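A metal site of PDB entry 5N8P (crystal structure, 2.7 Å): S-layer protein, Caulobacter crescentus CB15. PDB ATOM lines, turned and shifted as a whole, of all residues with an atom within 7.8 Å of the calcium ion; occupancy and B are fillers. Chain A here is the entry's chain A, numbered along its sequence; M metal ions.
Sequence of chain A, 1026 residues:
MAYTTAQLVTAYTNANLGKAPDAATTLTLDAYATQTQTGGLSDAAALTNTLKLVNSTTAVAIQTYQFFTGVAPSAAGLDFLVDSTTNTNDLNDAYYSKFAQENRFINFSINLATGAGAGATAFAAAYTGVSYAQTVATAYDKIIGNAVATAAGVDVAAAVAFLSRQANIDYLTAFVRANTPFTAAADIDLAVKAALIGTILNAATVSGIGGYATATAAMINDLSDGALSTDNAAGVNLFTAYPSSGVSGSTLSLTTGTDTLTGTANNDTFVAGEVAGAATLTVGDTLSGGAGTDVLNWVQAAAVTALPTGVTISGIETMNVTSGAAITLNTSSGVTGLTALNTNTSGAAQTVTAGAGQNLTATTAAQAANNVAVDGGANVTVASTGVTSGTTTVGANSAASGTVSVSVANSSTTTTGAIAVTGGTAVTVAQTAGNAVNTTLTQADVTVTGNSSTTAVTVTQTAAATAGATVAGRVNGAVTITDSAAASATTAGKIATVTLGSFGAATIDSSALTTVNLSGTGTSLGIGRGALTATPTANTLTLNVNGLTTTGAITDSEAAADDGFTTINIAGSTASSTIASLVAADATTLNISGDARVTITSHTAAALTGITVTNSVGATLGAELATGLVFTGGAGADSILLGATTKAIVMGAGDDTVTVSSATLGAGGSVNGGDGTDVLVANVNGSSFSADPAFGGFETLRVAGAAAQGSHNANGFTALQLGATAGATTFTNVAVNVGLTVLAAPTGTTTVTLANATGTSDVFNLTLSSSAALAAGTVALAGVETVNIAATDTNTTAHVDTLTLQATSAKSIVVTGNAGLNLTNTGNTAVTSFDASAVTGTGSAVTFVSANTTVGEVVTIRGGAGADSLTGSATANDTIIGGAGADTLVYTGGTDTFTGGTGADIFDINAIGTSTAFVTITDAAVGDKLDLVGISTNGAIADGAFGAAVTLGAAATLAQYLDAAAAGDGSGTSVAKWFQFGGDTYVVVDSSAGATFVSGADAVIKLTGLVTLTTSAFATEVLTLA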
ATOM      1  N   SER A 253       6.112 -37.642  -0.800  1.00  0.00           N
ATOM      2  CA  SER A 253       6.627 -36.725   0.201  1.00  0.00           C
ATOM      3  C   SER A 253       6.903 -35.300  -0.284  1.00  0.00           C
ATOM      4  O   SER A 253       7.717 -35.120  -1.173  1.00  0.00           O
ATOM      5  CB  SER A 253       7.926 -37.276   0.750  1.00  0.00           C
ATOM      6  OG  SER A 253       7.643 -38.133   1.809  1.00  0.00           O
ATOM      7  N   LEU A 254       6.290 -34.316   0.381  1.00  0.00           N
ATOM      8  CA  LEU A 254       6.593 -32.906   0.135  1.00  0.00           C
ATOM      9  C   LEU A 254       7.939 -32.530   0.729  1.00  0.00           C
ATOM     10  O   LEU A 254       8.350 -33.131   1.704  1.00  0.00           O
ATOM     11  CB  LEU A 254       5.512 -31.996   0.717  1.00  0.00           C
ATOM     12  CG  LEU A 254       4.274 -31.681  -0.149  1.00  0.00           C
ATOM     13  CD1 LEU A 254       3.343 -32.861  -0.221  1.00  0.00           C
ATOM     14  CD2 LEU A 254       3.522 -30.492   0.421  1.00  0.00           C
ATOM     15  N   THR A 255       8.635 -31.554   0.132  1.00  0.00           N
ATOM     16  CA  THR A 255       9.935 -31.040   0.609  1.00  0.00           C
ATOM     17  C   THR A 255       9.853 -29.592   1.039  1.00  0.00           C
ATOM     18  O   THR A 255       8.822 -28.965   0.838  1.00  0.00           O
ATOM     19  CB  THR A 255      11.012 -31.101  -0.471  1.00  0.00           C
ATOM     20  OG1 THR A 255      10.809 -30.001  -1.371  1.00  0.00           O
ATOM     21  CG2 THR A 255      10.947 -32.444  -1.223  1.00  0.00           C
ATOM     22  N   THR A 256      10.921 -29.026   1.577  1.00  0.00           N
ATOM     23  CA  THR A 256      10.863 -27.602   1.956  1.00  0.00           C
ATOM     24  C   THR A 256      10.855 -26.689   0.707  1.00  0.00           C
ATOM     25  O   THR A 256      10.840 -25.457   0.856  1.00  0.00           O
ATOM     26  CB  THR A 256      12.020 -27.162   2.877  1.00  0.00           C
ATOM     27  OG1 THR A 256      13.249 -27.334   2.197  1.00  0.00           O
ATOM     28  CG2 THR A 256      12.092 -28.025   4.107  1.00  0.00           C
ATOM     29  N   GLY A 257      10.822 -27.272  -0.488  1.00  0.00           N
ATOM     30  CA  GLY A 257      10.737 -26.508  -1.745  1.00  0.00           C
ATOM     31  C   GLY A 257       9.351 -26.255  -2.379  1.00  0.00           C
ATOM     32  O   GLY A 257       8.347 -26.162  -1.688  1.00  0.00           O
ATOM     33  N   THR A 258       9.318 -26.128  -3.703  1.00  0.00           N
ATOM     34  CA  THR A 258       8.082 -26.111  -4.427  1.00  0.00           C
ATOM     35  C   THR A 258       7.863 -27.446  -5.103  1.00  0.00           C
ATOM     36  O   THR A 258       8.609 -27.841  -5.985  1.00  0.00           O
ATOM     37  CB  THR A 258       8.048 -24.944  -5.440  1.00  0.00           C
ATOM     38  OG1 THR A 258       8.068 -23.731  -4.705  1.00  0.00           O
ATOM     39  CG2 THR A 258       6.786 -24.996  -6.275  1.00  0.00           C
ATOM     40  N   ASP A 259       6.800 -28.138  -4.669  1.00  0.00           N
ATOM     41  CA  ASP A 259       6.555 -29.490  -5.137  1.00  0.00           C
ATOM     42  C   ASP A 259       5.452 -29.517  -6.155  1.00  0.00           C
ATOM     43  O   ASP A 259       4.454 -28.812  -6.040  1.00  0.00           O
ATOM     44  CB  ASP A 259       6.229 -30.370  -3.946  1.00  0.00           C
ATOM     45  CG  ASP A 259       7.295 -30.275  -2.847  1.00  0.00           C
ATOM     46  OD1 ASP A 259       8.425 -30.823  -3.030  1.00  0.00           O
ATOM     47  OD2 ASP A 259       7.041 -29.600  -1.835  1.00  0.00           O
ATOM     48  N   THR A 260       5.629 -30.361  -7.168  1.00  0.00           N
ATOM     49  CA  THR A 260       4.607 -30.602  -8.171  1.00  0.00           C
ATOM     50  C   THR A 260       4.330 -32.110  -8.218  1.00  0.00           C
ATOM     51  O   THR A 260       4.961 -32.869  -8.956  1.00  0.00           O
ATOM     52  CB  THR A 260       4.973 -29.983  -9.535  1.00  0.00           C
ATOM     53  OG1 THR A 260       5.380 -28.615  -9.328  1.00  0.00           O
ATOM     54  CG2 THR A 260       3.774 -30.007 -10.496  1.00  0.00           C
ATOM     55  N   LEU A 261       3.362 -32.546  -7.416  1.00  0.00           N
ATOM     56  CA  LEU A 261       3.139 -33.957  -7.170  1.00  0.00           C
ATOM     57  C   LEU A 261       1.817 -34.413  -7.744  1.00  0.00           C
ATOM     58  O   LEU A 261       0.798 -33.734  -7.599  1.00  0.00           O
ATOM     59  CB  LEU A 261       3.238 -34.258  -5.680  1.00  0.00           C
ATOM     60  CG  LEU A 261       4.541 -33.906  -4.970  1.00  0.00           C
ATOM     61  CD1 LEU A 261       4.505 -34.237  -3.484  1.00  0.00           C
ATOM     62  CD2 LEU A 261       5.785 -34.520  -5.651  1.00  0.00           C
ATOM     63  N   ALA A 272       2.913 -34.199   4.142  1.00  0.00           N
ATOM     64  CA  ALA A 272       3.392 -32.846   4.265  1.00  0.00           C
ATOM     65  C   ALA A 272       3.895 -32.570   5.672  1.00  0.00           C
ATOM     66  O   ALA A 272       3.437 -31.658   6.353  1.00  0.00           O
ATOM     67  CB  ALA A 272       2.328 -31.876   3.867  1.00  0.00           C
ATOM     68  N   ALA A 279       8.673 -26.752   7.898  1.00  0.00           N
ATOM     69  CA  ALA A 279       7.422 -27.124   7.226  1.00  0.00           C
ATOM     70  C   ALA A 279       7.624 -27.570   5.777  1.00  0.00           C
ATOM     71  O   ALA A 279       8.514 -27.011   5.109  1.00  0.00           O
ATOM     72  CB  ALA A 279       6.474 -25.955   7.265  1.00  0.00           C
ATOM     73  N   THR A 280       6.862 -28.550   5.301  1.00  0.00           N
ATOM     74  CA  THR A 280       6.981 -28.930   3.873  1.00  0.00           C
ATOM     75  C   THR A 280       5.818 -28.538   2.958  1.00  0.00           C
ATOM     76  O   THR A 280       5.907 -28.686   1.731  1.00  0.00           O
ATOM     77  CB  THR A 280       7.378 -30.400   3.623  1.00  0.00           C
ATOM     78  OG1 THR A 280       6.287 -31.276   3.946  1.00  0.00           O
ATOM     79  CG2 THR A 280       8.613 -30.766   4.397  1.00  0.00           C
ATOM     80  N   LEU A 281       4.723 -28.054   3.528  1.00  0.00           N
ATOM     81  CA  LEU A 281       3.718 -27.378   2.714  1.00  0.00           C
ATOM     82  C   LEU A 281       4.114 -25.911   2.666  1.00  0.00           C
ATOM     83  O   LEU A 281       4.094 -25.210   3.681  1.00  0.00           O
ATOM     84  CB  LEU A 281       2.302 -27.608   3.204  1.00  0.00           C
ATOM     85  CG  LEU A 281       1.202 -27.323   2.200  1.00  0.00           C
ATOM     86  CD1 LEU A 281       0.899 -28.502   1.296  1.00  0.00           C
ATOM     87  CD2 LEU A 281      -0.064 -26.969   2.947  1.00  0.00           C
ATOM     88  N   THR A 282       4.526 -25.480   1.484  1.00  0.00           N
ATOM     89  CA  THR A 282       5.214 -24.193   1.278  1.00  0.00           C
ATOM     90  C   THR A 282       4.780 -23.565  -0.022  1.00  0.00           C
ATOM     91  O   THR A 282       4.085 -24.207  -0.838  1.00  0.00           O
ATOM     92  CB  THR A 282       6.715 -24.409   1.150  1.00  0.00           C
ATOM     93  OG1 THR A 282       6.926 -25.581   0.362  1.00  0.00           O
ATOM     94  CG2 THR A 282       7.369 -24.611   2.524  1.00  0.00           C
ATOM     95  N   VAL A 283       5.228 -22.333  -0.258  1.00  0.00           N
ATOM     96  CA  VAL A 283       4.791 -21.554  -1.409  1.00  0.00           C
ATOM     97  C   VAL A 283       4.860 -22.298  -2.747  1.00  0.00           C
ATOM     98  O   VAL A 283       5.841 -22.932  -3.045  1.00  0.00           O
ATOM     99  CB  VAL A 283       5.371 -20.091  -1.414  1.00  0.00           C
ATOM    100  CG1 VAL A 283       5.928 -19.658  -0.048  1.00  0.00           C
ATOM    101  CG2 VAL A 283       6.520 -19.966  -2.337  1.00  0.00           C
ATOM    102  N   GLY A 284       3.755 -22.258  -3.502  1.00  0.00           N
ATOM    103  CA  GLY A 284       3.672 -22.803  -4.857  1.00  0.00           C
ATOM    104  C   GLY A 284       3.412 -24.292  -4.969  1.00  0.00           C
ATOM    105  O   GLY A 284       3.172 -24.775  -6.098  1.00  0.00           O
ATOM    106  N   ASP A 285       3.480 -25.013  -3.853  1.00  0.00           N
ATOM    107  CA  ASP A 285       3.197 -26.441  -3.821  1.00  0.00           C
ATOM    108  C   ASP A 285       1.895 -26.765  -4.560  1.00  0.00           C
ATOM    109  O   ASP A 285       0.837 -26.237  -4.214  1.00  0.00           O
ATOM    110  CB  ASP A 285       3.089 -26.957  -2.379  1.00  0.00           C
ATOM    111  CG  ASP A 285       4.428 -27.141  -1.677  1.00  0.00           C
ATOM    112  OD1 ASP A 285       4.420 -27.307  -0.435  1.00  0.00           O
ATOM    113  OD2 ASP A 285       5.504 -27.148  -2.324  1.00  0.00           O
ATOM    114  N   THR A 286       1.950 -27.612  -5.578  1.00  0.00           N
ATOM    115  CA  THR A 286       0.688 -28.038  -6.193  1.00  0.00           C
ATOM    116  C   THR A 286       0.565 -29.554  -6.202  1.00  0.00           C
ATOM    117  O   THR A 286       1.452 -30.273  -6.684  1.00  0.00           O
ATOM    118  CB  THR A 286       0.392 -27.375  -7.581  1.00  0.00           C
ATOM    119  OG1 THR A 286       1.221 -27.958  -8.577  1.00  0.00           O
ATOM    120  CG2 THR A 286       0.558 -25.814  -7.597  1.00  0.00           C
ATOM    121  N   LEU A 287      -0.556 -30.027  -5.636  1.00  0.00           N
ATOM    122  CA  LEU A 287      -0.818 -31.463  -5.457  1.00  0.00           C
ATOM    123  C   LEU A 287      -2.053 -31.908  -6.216  1.00  0.00           C
ATOM    124  O   LEU A 287      -3.053 -31.197  -6.250  1.00  0.00           O
ATOM    125  CB  LEU A 287      -0.897 -31.832  -3.968  1.00  0.00           C
ATOM    126  CG  LEU A 287       0.117 -31.235  -3.007  1.00  0.00           C
ATOM    127  CD1 LEU A 287      -0.343 -31.353  -1.559  1.00  0.00           C
ATOM    128  CD2 LEU A 287       1.498 -31.838  -3.267  1.00  0.00           C
ATOM    129  N   VAL A 311      -0.357 -22.321  -3.278  1.00  0.00           N
ATOM    130  CA  VAL A 311      -0.703 -23.705  -2.965  1.00  0.00           C
ATOM    131  C   VAL A 311      -2.065 -24.036  -3.558  1.00  0.00           C
ATOM    132  O   VAL A 311      -3.002 -23.252  -3.405  1.00  0.00           O
ATOM    133  CB  VAL A 311      -0.632 -24.003  -1.445  1.00  0.00           C
ATOM    134  CG1 VAL A 311      -1.237 -25.382  -1.104  1.00  0.00           C
ATOM    135  CG2 VAL A 311       0.803 -23.965  -0.958  1.00  0.00           C
HETATM  136 CA    CA M   1       6.852 -27.904  -0.289  1.00  0.00          CA
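N of Thr 286 is in hydrogen-bond range of O of Asp 259 (2.8 Å). OG1 of Thr 255 lies within hydrogen-bond range of N of Gly 257, 2.9 Å away.
Of the 20 residues printed, 6 come within 4 Å of the calcium ion. The nearest printed residue that does not touch the calcium ion is Leu 254 (4.3 Å).
The calcium ion is bound by OD2 of Asp 259 (2.3 Å), O of Thr 280 (2.4 Å), OG1 of Thr 282 (2.4 Å), O of Thr 255 (2.5 Å), OD1 of Asp 285 (2.5 Å), OD2 of Asp 285 (2.6 Å) and O of Gly 257 (2.7 Å).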
